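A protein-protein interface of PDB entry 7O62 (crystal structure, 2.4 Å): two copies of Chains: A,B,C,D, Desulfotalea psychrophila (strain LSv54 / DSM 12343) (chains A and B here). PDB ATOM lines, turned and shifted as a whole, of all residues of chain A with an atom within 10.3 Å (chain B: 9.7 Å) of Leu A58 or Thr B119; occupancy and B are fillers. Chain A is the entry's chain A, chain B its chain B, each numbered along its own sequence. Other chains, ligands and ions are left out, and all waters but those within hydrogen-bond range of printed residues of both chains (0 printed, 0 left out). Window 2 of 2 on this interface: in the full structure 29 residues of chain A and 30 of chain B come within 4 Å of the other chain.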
ATOM      1  N   PHE A  17       5.210   7.293  24.401  1.00  0.00           N
ATOM      2  CA  PHE A  17       3.987   7.594  23.668  1.00  0.00           C
ATOM      3  C   PHE A  17       2.901   6.527  23.776  1.00  0.00           C
ATOM      4  O   PHE A  17       1.750   6.817  23.433  1.00  0.00           O
ATOM      5  CB  PHE A  17       4.317   7.844  22.187  1.00  0.00           C
ATOM      6  CG  PHE A  17       5.433   8.824  21.990  1.00  0.00           C
ATOM      7  CD1 PHE A  17       5.213  10.184  22.163  1.00  0.00           C
ATOM      8  CD2 PHE A  17       6.710   8.387  21.669  1.00  0.00           C
ATOM      9  CE1 PHE A  17       6.243  11.089  22.003  1.00  0.00           C
ATOM     10  CE2 PHE A  17       7.742   9.288  21.512  1.00  0.00           C
ATOM     11  CZ  PHE A  17       7.507  10.644  21.676  1.00  0.00           C
ATOM     12  N   LEU A  54      -6.223  19.196  32.105  1.00  0.00           N
ATOM     13  CA  LEU A  54      -6.281  19.942  30.853  1.00  0.00           C
ATOM     14  C   LEU A  54      -6.699  21.392  31.091  1.00  0.00           C
ATOM     15  O   LEU A  54      -6.716  21.868  32.226  1.00  0.00           O
ATOM     16  CB  LEU A  54      -7.237  19.271  29.863  1.00  0.00           C
ATOM     17  CG  LEU A  54      -6.632  18.180  28.974  1.00  0.00           C
ATOM     18  CD1 LEU A  54      -5.566  18.773  28.034  1.00  0.00           C
ATOM     19  CD2 LEU A  54      -6.084  17.010  29.794  1.00  0.00           C
ATOM     20  N   GLY A  55      -7.044  22.090  30.011  1.00  0.00           N
ATOM     21  CA  GLY A  55      -7.302  23.514  30.092  1.00  0.00           C
ATOM     22  C   GLY A  55      -6.024  24.286  29.864  1.00  0.00           C
ATOM     23  O   GLY A  55      -5.739  25.262  30.568  1.00  0.00           O
ATOM     24  N   THR A  56      -5.249  23.854  28.872  1.00  0.00           N
ATOM     25  CA  THR A  56      -3.874  24.309  28.687  1.00  0.00           C
ATOM     26  C   THR A  56      -3.670  24.743  27.241  1.00  0.00           C
ATOM     27  O   THR A  56      -3.847  23.920  26.320  1.00  0.00           O
ATOM     28  CB  THR A  56      -2.900  23.191  29.078  1.00  0.00           C
ATOM     29  OG1 THR A  56      -3.490  21.915  28.782  1.00  0.00           O
ATOM     30  CG2 THR A  56      -2.578  23.254  30.567  1.00  0.00           C
ATOM     31  N   PRO A  57      -3.300  26.002  26.982  1.00  0.00           N
ATOM     32  CA  PRO A  57      -3.050  26.421  25.596  1.00  0.00           C
ATOM     33  C   PRO A  57      -1.749  25.812  25.094  1.00  0.00           C
ATOM     34  O   PRO A  57      -0.723  25.849  25.779  1.00  0.00           O
ATOM     35  CB  PRO A  57      -2.969  27.949  25.684  1.00  0.00           C
ATOM     36  CG  PRO A  57      -2.793  28.275  27.147  1.00  0.00           C
ATOM     37  CD  PRO A  57      -2.867  27.014  27.957  1.00  0.00           C
ATOM     38  N   LEU A  58      -1.807  25.250  23.887  1.00  0.00           N
ATOM     39  CA  LEU A  58      -0.751  24.362  23.412  1.00  0.00           C
ATOM     40  C   LEU A  58       0.629  24.991  23.543  1.00  0.00           C
ATOM     41  O   LEU A  58       1.567  24.360  24.047  1.00  0.00           O
ATOM     42  CB  LEU A  58      -1.021  23.977  21.959  1.00  0.00           C
ATOM     43  CG  LEU A  58      -0.124  22.864  21.421  1.00  0.00           C
ATOM     44  CD1 LEU A  58      -0.412  21.570  22.172  1.00  0.00           C
ATOM     45  CD2 LEU A  58      -0.310  22.703  19.918  1.00  0.00           C
ATOM     46  N   LYS A  59       0.769  26.246  23.107  1.00  0.00           N
ATOM     47  CA  LYS A  59       2.103  26.824  22.960  1.00  0.00           C
ATOM     48  C   LYS A  59       2.806  26.959  24.306  1.00  0.00           C
ATOM     49  O   LYS A  59       4.004  26.670  24.413  1.00  0.00           O
ATOM     50  CB  LYS A  59       2.017  28.173  22.245  1.00  0.00           C
ATOM     51  CG  LYS A  59       1.372  28.125  20.845  1.00  0.00           C
ATOM     52  CD  LYS A  59       2.230  27.357  19.814  1.00  0.00           C
ATOM     53  CE  LYS A  59       1.780  25.893  19.622  1.00  0.00           C
ATOM     54  NZ  LYS A  59       2.833  25.004  19.023  1.00  0.00           N
ATOM     55  N   VAL A  60       2.077  27.372  25.349  1.00  0.00           N
ATOM     56  CA  VAL A  60       2.681  27.471  26.674  1.00  0.00           C
ATOM     57  C   VAL A  60       2.844  26.101  27.330  1.00  0.00           C
ATOM     58  O   VAL A  60       3.694  25.937  28.224  1.00  0.00           O
ATOM     59  CB  VAL A  60       1.870  28.401  27.588  1.00  0.00           C
ATOM     60  CG1 VAL A  60       1.407  29.637  26.810  1.00  0.00           C
ATOM     61  CG2 VAL A  60       0.698  27.653  28.236  1.00  0.00           C
ATOM     62  N   ALA A  61       2.054  25.110  26.906  1.00  0.00           N
ATOM     63  CA  ALA A  61       2.271  23.742  27.360  1.00  0.00           C
ATOM     64  C   ALA A  61       3.612  23.223  26.862  1.00  0.00           C
ATOM     65  O   ALA A  61       4.477  22.840  27.656  1.00  0.00           O
ATOM     66  CB  ALA A  61       1.121  22.851  26.891  1.00  0.00           C
ATOM     67  N   GLU A  62       3.805  23.220  25.536  1.00  0.00           N
ATOM     68  CA  GLU A  62       5.081  22.789  24.968  1.00  0.00           C
ATOM     69  C   GLU A  62       6.248  23.522  25.618  1.00  0.00           C
ATOM     70  O   GLU A  62       7.267  22.906  25.945  1.00  0.00           O
ATOM     71  CB  GLU A  62       5.092  23.004  23.450  1.00  0.00           C
ATOM     72  CG  GLU A  62       3.761  22.730  22.772  1.00  0.00           C
ATOM     73  CD  GLU A  62       3.718  23.165  21.314  1.00  0.00           C
ATOM     74  OE1 GLU A  62       4.076  24.330  21.010  1.00  0.00           O
ATOM     75  OE2 GLU A  62       3.308  22.341  20.469  1.00  0.00           O
ATOM     76  N   LYS A  63       6.098  24.827  25.857  1.00  0.00           N
ATOM     77  CA  LYS A  63       7.188  25.606  26.436  1.00  0.00           C
ATOM     78  C   LYS A  63       7.579  25.084  27.818  1.00  0.00           C
ATOM     79  O   LYS A  63       8.769  24.981  28.135  1.00  0.00           O
ATOM     80  CB  LYS A  63       6.795  27.083  26.507  1.00  0.00           C
ATOM     81  CG  LYS A  63       7.926  28.001  26.978  1.00  0.00           C
ATOM     82  CD  LYS A  63       7.817  28.300  28.477  1.00  0.00           C
ATOM     83  CE  LYS A  63       8.517  29.593  28.870  1.00  0.00           C
ATOM     84  NZ  LYS A  63       7.901  30.212  30.085  1.00  0.00           N
ATOM     85  N   SER A  64       6.590  24.748  28.651  1.00  0.00           N
ATOM     86  CA  SER A  64       6.866  24.322  30.018  1.00  0.00           C
ATOM     87  C   SER A  64       7.447  22.914  30.073  1.00  0.00           C
ATOM     88  O   SER A  64       8.374  22.651  30.854  1.00  0.00           O
ATOM     89  CB  SER A  64       5.587  24.395  30.841  1.00  0.00           C
ATOM     90  OG  SER A  64       4.571  23.661  30.187  1.00  0.00           O
ATOM     91  N   ILE A  65       6.898  21.991  29.274  1.00  0.00           N
ATOM     92  CA  ILE A  65       7.514  20.671  29.128  1.00  0.00           C
ATOM     93  C   ILE A  65       8.962  20.824  28.672  1.00  0.00           C
ATOM     94  O   ILE A  65       9.887  20.228  29.241  1.00  0.00           O
ATOM     95  CB  ILE A  65       6.703  19.807  28.142  1.00  0.00           C
ATOM     96  CG1 ILE A  65       5.469  19.203  28.816  1.00  0.00           C
ATOM     97  CG2 ILE A  65       7.564  18.690  27.569  1.00  0.00           C
ATOM     98  CD1 ILE A  65       4.484  18.568  27.815  1.00  0.00           C
ATOM     99  N   TYR A  66       9.172  21.655  27.650  1.00  0.00           N
ATOM    100  CA  TYR A  66      10.504  21.901  27.110  1.00  0.00           C
ATOM    101  C   TYR A  66      11.444  22.479  28.168  1.00  0.00           C
ATOM    102  O   TYR A  66      12.531  21.935  28.414  1.00  0.00           O
ATOM    103  CB  TYR A  66      10.376  22.852  25.923  1.00  0.00           C
ATOM    104  CG  TYR A  66      11.668  23.308  25.297  1.00  0.00           C
ATOM    105  CD1 TYR A  66      12.407  22.453  24.476  1.00  0.00           C
ATOM    106  CD2 TYR A  66      12.127  24.606  25.478  1.00  0.00           C
ATOM    107  CE1 TYR A  66      13.565  22.882  23.871  1.00  0.00           C
ATOM    108  CE2 TYR A  66      13.290  25.036  24.880  1.00  0.00           C
ATOM    109  CZ  TYR A  66      13.997  24.174  24.077  1.00  0.00           C
ATOM    110  OH  TYR A  66      15.154  24.598  23.488  1.00  0.00           O
ATOM    111  N   GLN B 110      10.092  22.750   7.068  1.00  0.00           N
ATOM    112  CA  GLN B 110       9.110  21.674   7.146  1.00  0.00           C
ATOM    113  C   GLN B 110       8.036  21.936   6.094  1.00  0.00           C
ATOM    114  O   GLN B 110       7.165  22.791   6.295  1.00  0.00           O
ATOM    115  CB  GLN B 110       8.511  21.600   8.545  1.00  0.00           C
ATOM    116  CG  GLN B 110       7.576  20.448   8.771  1.00  0.00           C
ATOM    117  CD  GLN B 110       7.316  20.223  10.237  1.00  0.00           C
ATOM    118  OE1 GLN B 110       7.796  19.260  10.816  1.00  0.00           O
ATOM    119  NE2 GLN B 110       6.548  21.111  10.843  1.00  0.00           N
ATOM    120  N   ARG B 114       3.144  15.274   7.254  1.00  0.00           N
ATOM    121  CA  ARG B 114       3.169  14.366   8.395  1.00  0.00           C
ATOM    122  C   ARG B 114       3.707  15.053   9.655  1.00  0.00           C
ATOM    123  O   ARG B 114       4.527  15.977   9.597  1.00  0.00           O
ATOM    124  CB  ARG B 114       4.010  13.128   8.065  1.00  0.00           C
ATOM    125  CG  ARG B 114       3.436  12.302   6.926  1.00  0.00           C
ATOM    126  CD  ARG B 114       4.397  11.251   6.429  1.00  0.00           C
ATOM    127  NE  ARG B 114       5.496  11.865   5.698  1.00  0.00           N
ATOM    128  CZ  ARG B 114       6.454  11.198   5.067  1.00  0.00           C
ATOM    129  NH1 ARG B 114       6.475   9.877   5.041  1.00  0.00           N
ATOM    130  NH2 ARG B 114       7.417  11.875   4.442  1.00  0.00           N
ATOM    131  N   ARG B 115       3.229  14.584  10.808  1.00  0.00           N
ATOM    132  CA  ARG B 115       3.661  15.092  12.102  1.00  0.00           C
ATOM    133  C   ARG B 115       3.852  13.923  13.063  1.00  0.00           C
ATOM    134  O   ARG B 115       3.395  12.803  12.808  1.00  0.00           O
ATOM    135  CB  ARG B 115       2.651  16.102  12.666  1.00  0.00           C
ATOM    136  CG  ARG B 115       2.590  17.404  11.889  1.00  0.00           C
ATOM    137  CD  ARG B 115       3.933  18.114  11.939  1.00  0.00           C
ATOM    138  NE  ARG B 115       3.788  19.524  11.612  1.00  0.00           N
ATOM    139  CZ  ARG B 115       3.692  19.991  10.375  1.00  0.00           C
ATOM    140  NH1 ARG B 115       3.807  19.194   9.327  1.00  0.00           N
ATOM    141  NH2 ARG B 115       3.473  21.291  10.187  1.00  0.00           N
ATOM    142  N   GLN B 116       4.550  14.190  14.171  1.00  0.00           N
ATOM    143  CA  GLN B 116       4.762  13.146  15.172  1.00  0.00           C
ATOM    144  C   GLN B 116       3.436  12.690  15.761  1.00  0.00           C
ATOM    145  O   GLN B 116       3.131  11.494  15.785  1.00  0.00           O
ATOM    146  CB  GLN B 116       5.676  13.634  16.296  1.00  0.00           C
ATOM    147  CG  GLN B 116       5.890  12.550  17.356  1.00  0.00           C
ATOM    148  CD  GLN B 116       6.887  12.922  18.448  1.00  0.00           C
ATOM    149  OE1 GLN B 116       8.067  12.549  18.376  1.00  0.00           O
ATOM    150  NE2 GLN B 116       6.401  13.578  19.510  1.00  0.00           N
ATOM    151  N   ALA B 117       2.648  13.635  16.255  1.00  0.00           N
ATOM    152  CA  ALA B 117       1.325  13.417  16.819  1.00  0.00           C
ATOM    153  C   ALA B 117       0.394  14.462  16.235  1.00  0.00           C
ATOM    154  O   ALA B 117       0.847  15.429  15.613  1.00  0.00           O
ATOM    155  CB  ALA B 117       1.358  13.515  18.356  1.00  0.00           C
ATOM    156  N   PRO B 118      -0.932  14.291  16.394  1.00  0.00           N
ATOM    157  CA  PRO B 118      -1.863  15.319  15.901  1.00  0.00           C
ATOM    158  C   PRO B 118      -1.544  16.716  16.420  1.00  0.00           C
ATOM    159  O   PRO B 118      -1.881  17.716  15.779  1.00  0.00           O
ATOM    160  CB  PRO B 118      -3.228  14.825  16.406  1.00  0.00           C
ATOM    161  CG  PRO B 118      -3.086  13.345  16.468  1.00  0.00           C
ATOM    162  CD  PRO B 118      -1.645  13.078  16.844  1.00  0.00           C
ATOM    163  N   THR B 119      -0.873  16.799  17.564  1.00  0.00           N
ATOM    164  CA  THR B 119      -0.585  18.079  18.195  1.00  0.00           C
ATOM    165  C   THR B 119       0.689  18.727  17.661  1.00  0.00           C
ATOM    166  O   THR B 119       1.154  19.712  18.239  1.00  0.00           O
ATOM    167  CB  THR B 119      -0.516  17.909  19.723  1.00  0.00           C
ATOM    168  OG1 THR B 119       0.184  19.014  20.305  1.00  0.00           O
ATOM    169  CG2 THR B 119       0.176  16.604  20.116  1.00  0.00           C
ATOM    170  N   GLY B 120       1.246  18.212  16.571  1.00  0.00           N
ATOM    171  CA  GLY B 120       2.406  18.814  15.936  1.00  0.00           C
ATOM    172  C   GLY B 120       3.707  18.087  16.223  1.00  0.00           C
ATOM    173  O   GLY B 120       3.741  16.917  16.617  1.00  0.00           O
ATOM    174  N   ASN B 121       4.804  18.809  16.014  1.00  0.00           N
ATOM    175  CA  ASN B 121       6.125  18.255  16.272  1.00  0.00           C
ATOM    176  C   ASN B 121       6.373  18.063  17.762  1.00  0.00           C
ATOM    177  O   ASN B 121       5.688  18.629  18.617  1.00  0.00           O
ATOM    178  CB  ASN B 121       7.206  19.157  15.687  1.00  0.00           C
ATOM    179  CG  ASN B 121       7.137  19.211  14.176  1.00  0.00           C
ATOM    180  OD1 ASN B 121       7.249  20.281  13.577  1.00  0.00           O
ATOM    181  ND2 ASN B 121       6.916  18.052  13.556  1.00  0.00           N
ATOM    182  N   ASN B 122       7.367  17.239  18.061  1.00  0.00           N
ATOM    183  CA  ASN B 122       7.788  17.043  19.440  1.00  0.00           C
ATOM    184  C   ASN B 122       8.084  18.394  20.095  1.00  0.00           C
ATOM    185  O   ASN B 122       8.593  19.306  19.430  1.00  0.00           O
ATOM    186  CB  ASN B 122       9.026  16.136  19.494  1.00  0.00           C
ATOM    187  CG  ASN B 122       9.390  15.725  20.906  1.00  0.00           C
ATOM    188  OD1 ASN B 122       9.902  16.527  21.681  1.00  0.00           O
ATOM    189  ND2 ASN B 122       9.124  14.474  21.247  1.00  0.00           N
ATOM    190  N   PRO B 123       7.748  18.570  21.381  1.00  0.00           N
ATOM    191  CA  PRO B 123       8.066  19.832  22.068  1.00  0.00           C
ATOM    192  C   PRO B 123       9.529  20.220  22.009  1.00  0.00           C
ATOM    193  O   PRO B 123       9.837  21.416  22.013  1.00  0.00           O
ATOM    194  CB  PRO B 123       7.635  19.558  23.514  1.00  0.00           C
ATOM    195  CG  PRO B 123       6.522  18.587  23.386  1.00  0.00           C
ATOM    196  CD  PRO B 123       6.814  17.735  22.156  1.00  0.00           C
ATOM    197  N   GLU B 126       9.795  21.686  18.317  1.00  0.00           N
ATOM    198  CA  GLU B 126       8.974  22.878  18.115  1.00  0.00           C
ATOM    199  C   GLU B 126       9.479  24.063  18.940  1.00  0.00           C
ATOM    200  O   GLU B 126       9.474  25.209  18.467  1.00  0.00           O
ATOM    201  CB  GLU B 126       7.515  22.547  18.463  1.00  0.00           C
ATOM    202  CG  GLU B 126       6.501  23.613  18.109  1.00  0.00           C
ATOM    203  CD  GLU B 126       6.249  23.713  16.608  1.00  0.00           C
ATOM    204  OE1 GLU B 126       6.220  22.657  15.927  1.00  0.00           O
ATOM    205  OE2 GLU B 126       6.079  24.854  16.106  1.00  0.00           O
ATOM    206  N   CYS B 127       9.924  23.813  20.173  1.00  0.00           N
ATOM    207  CA  CYS B 127      10.353  24.902  21.033  1.00  0.00           C
ATOM    208  C   CYS B 127      11.833  25.241  20.906  1.00  0.00           C
ATOM    209  O   CYS B 127      12.255  26.271  21.438  1.00  0.00           O
ATOM    210  CB  CYS B 127      10.052  24.582  22.488  1.00  0.00           C
ATOM    211  SG  CYS B 127       8.314  24.411  22.842  1.00  0.00           S
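The side-chain sulfur of Cys B127 sits at hydrogen-bond distance from the backbone NH of Lys A63. The backbone carbonyl oxygen (O) of Glu A62 sits close to the side-chain sulfur (SG) of Cys B127 (3.6 Å).
The side-chain amino group of Lys A59 lies within salt-bridge range of the side-chain carboxylate of Glu A62 (2.4 Å). SG of Cys B127 lies close to O of Pro B123 (3.5 Å). The side-chain carboxylate (OE1) of Glu B126 sits close to the side-chain amide oxygen (OD1) of Asn B121, at 3.5 Å. The side-chain amide nitrogen (NE2) of Gln B116 lies close to the side-chain amide nitrogen (ND2) of Asn B122, 3.4 Å away.
Among the printed residues, merely in contact across the chains: Phe A17 with Gln B116 (3.5 Å), Leu A58 with Thr B119 (3.2 Å), Glu A62 with Glu B126 (3.8 Å), Tyr A66 with Pro B123 (3.7 Å) and Tyr A66 with Cys B127 (3.5 Å).
Leu A58 touches just one residue of chain B: Thr B119. Thr B119 touches just one residue of chain A: Leu A58. No residue of chain B comes within 4 Å of Pro A57. No residue of chain B comes within 4 Å of Lys A59. No residue of chain B comes within 4 Å of Ala A61. No residue of chain A comes within 4 Å of Ala B117. No residue of chain A comes within 4 Å of Gly B120. Of the printed residues of chain A, Pro B123 touches Tyr A66 (3.7 Å). Of the printed residues of chain A, Gln B116 touches Phe A17 (3.5 Å). Of the printed residues of chain B, Lys A63 touches Cys B127 (3.8 Å). Of the printed residues of chain A, Cys B127 touches Glu A62 (3.6 Å), Lys A63 (3.8 Å) and Tyr A66 (3.5 Å). The nearest residue of chain B that does not touch Leu A58 is Gly B120 (5.8 Å). The nearest printed residue of chain A that does not touch Pro B123 is Ile A65 (4.1 Å).
Of the 13 printed residues of chain B, 5 touch a printed residue of chain A. Printed residues of chain B that touch a printed residue of chain A: Gln B116, Thr B119, Pro B123, Glu B126 and Cys B127. Among the printed residues, 7 pairs touch across the chains.
No position is printed for both chains. Of the 7 pairs that touch across the chains among the printed residues, none has its exchanged pair printed and touching as well.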
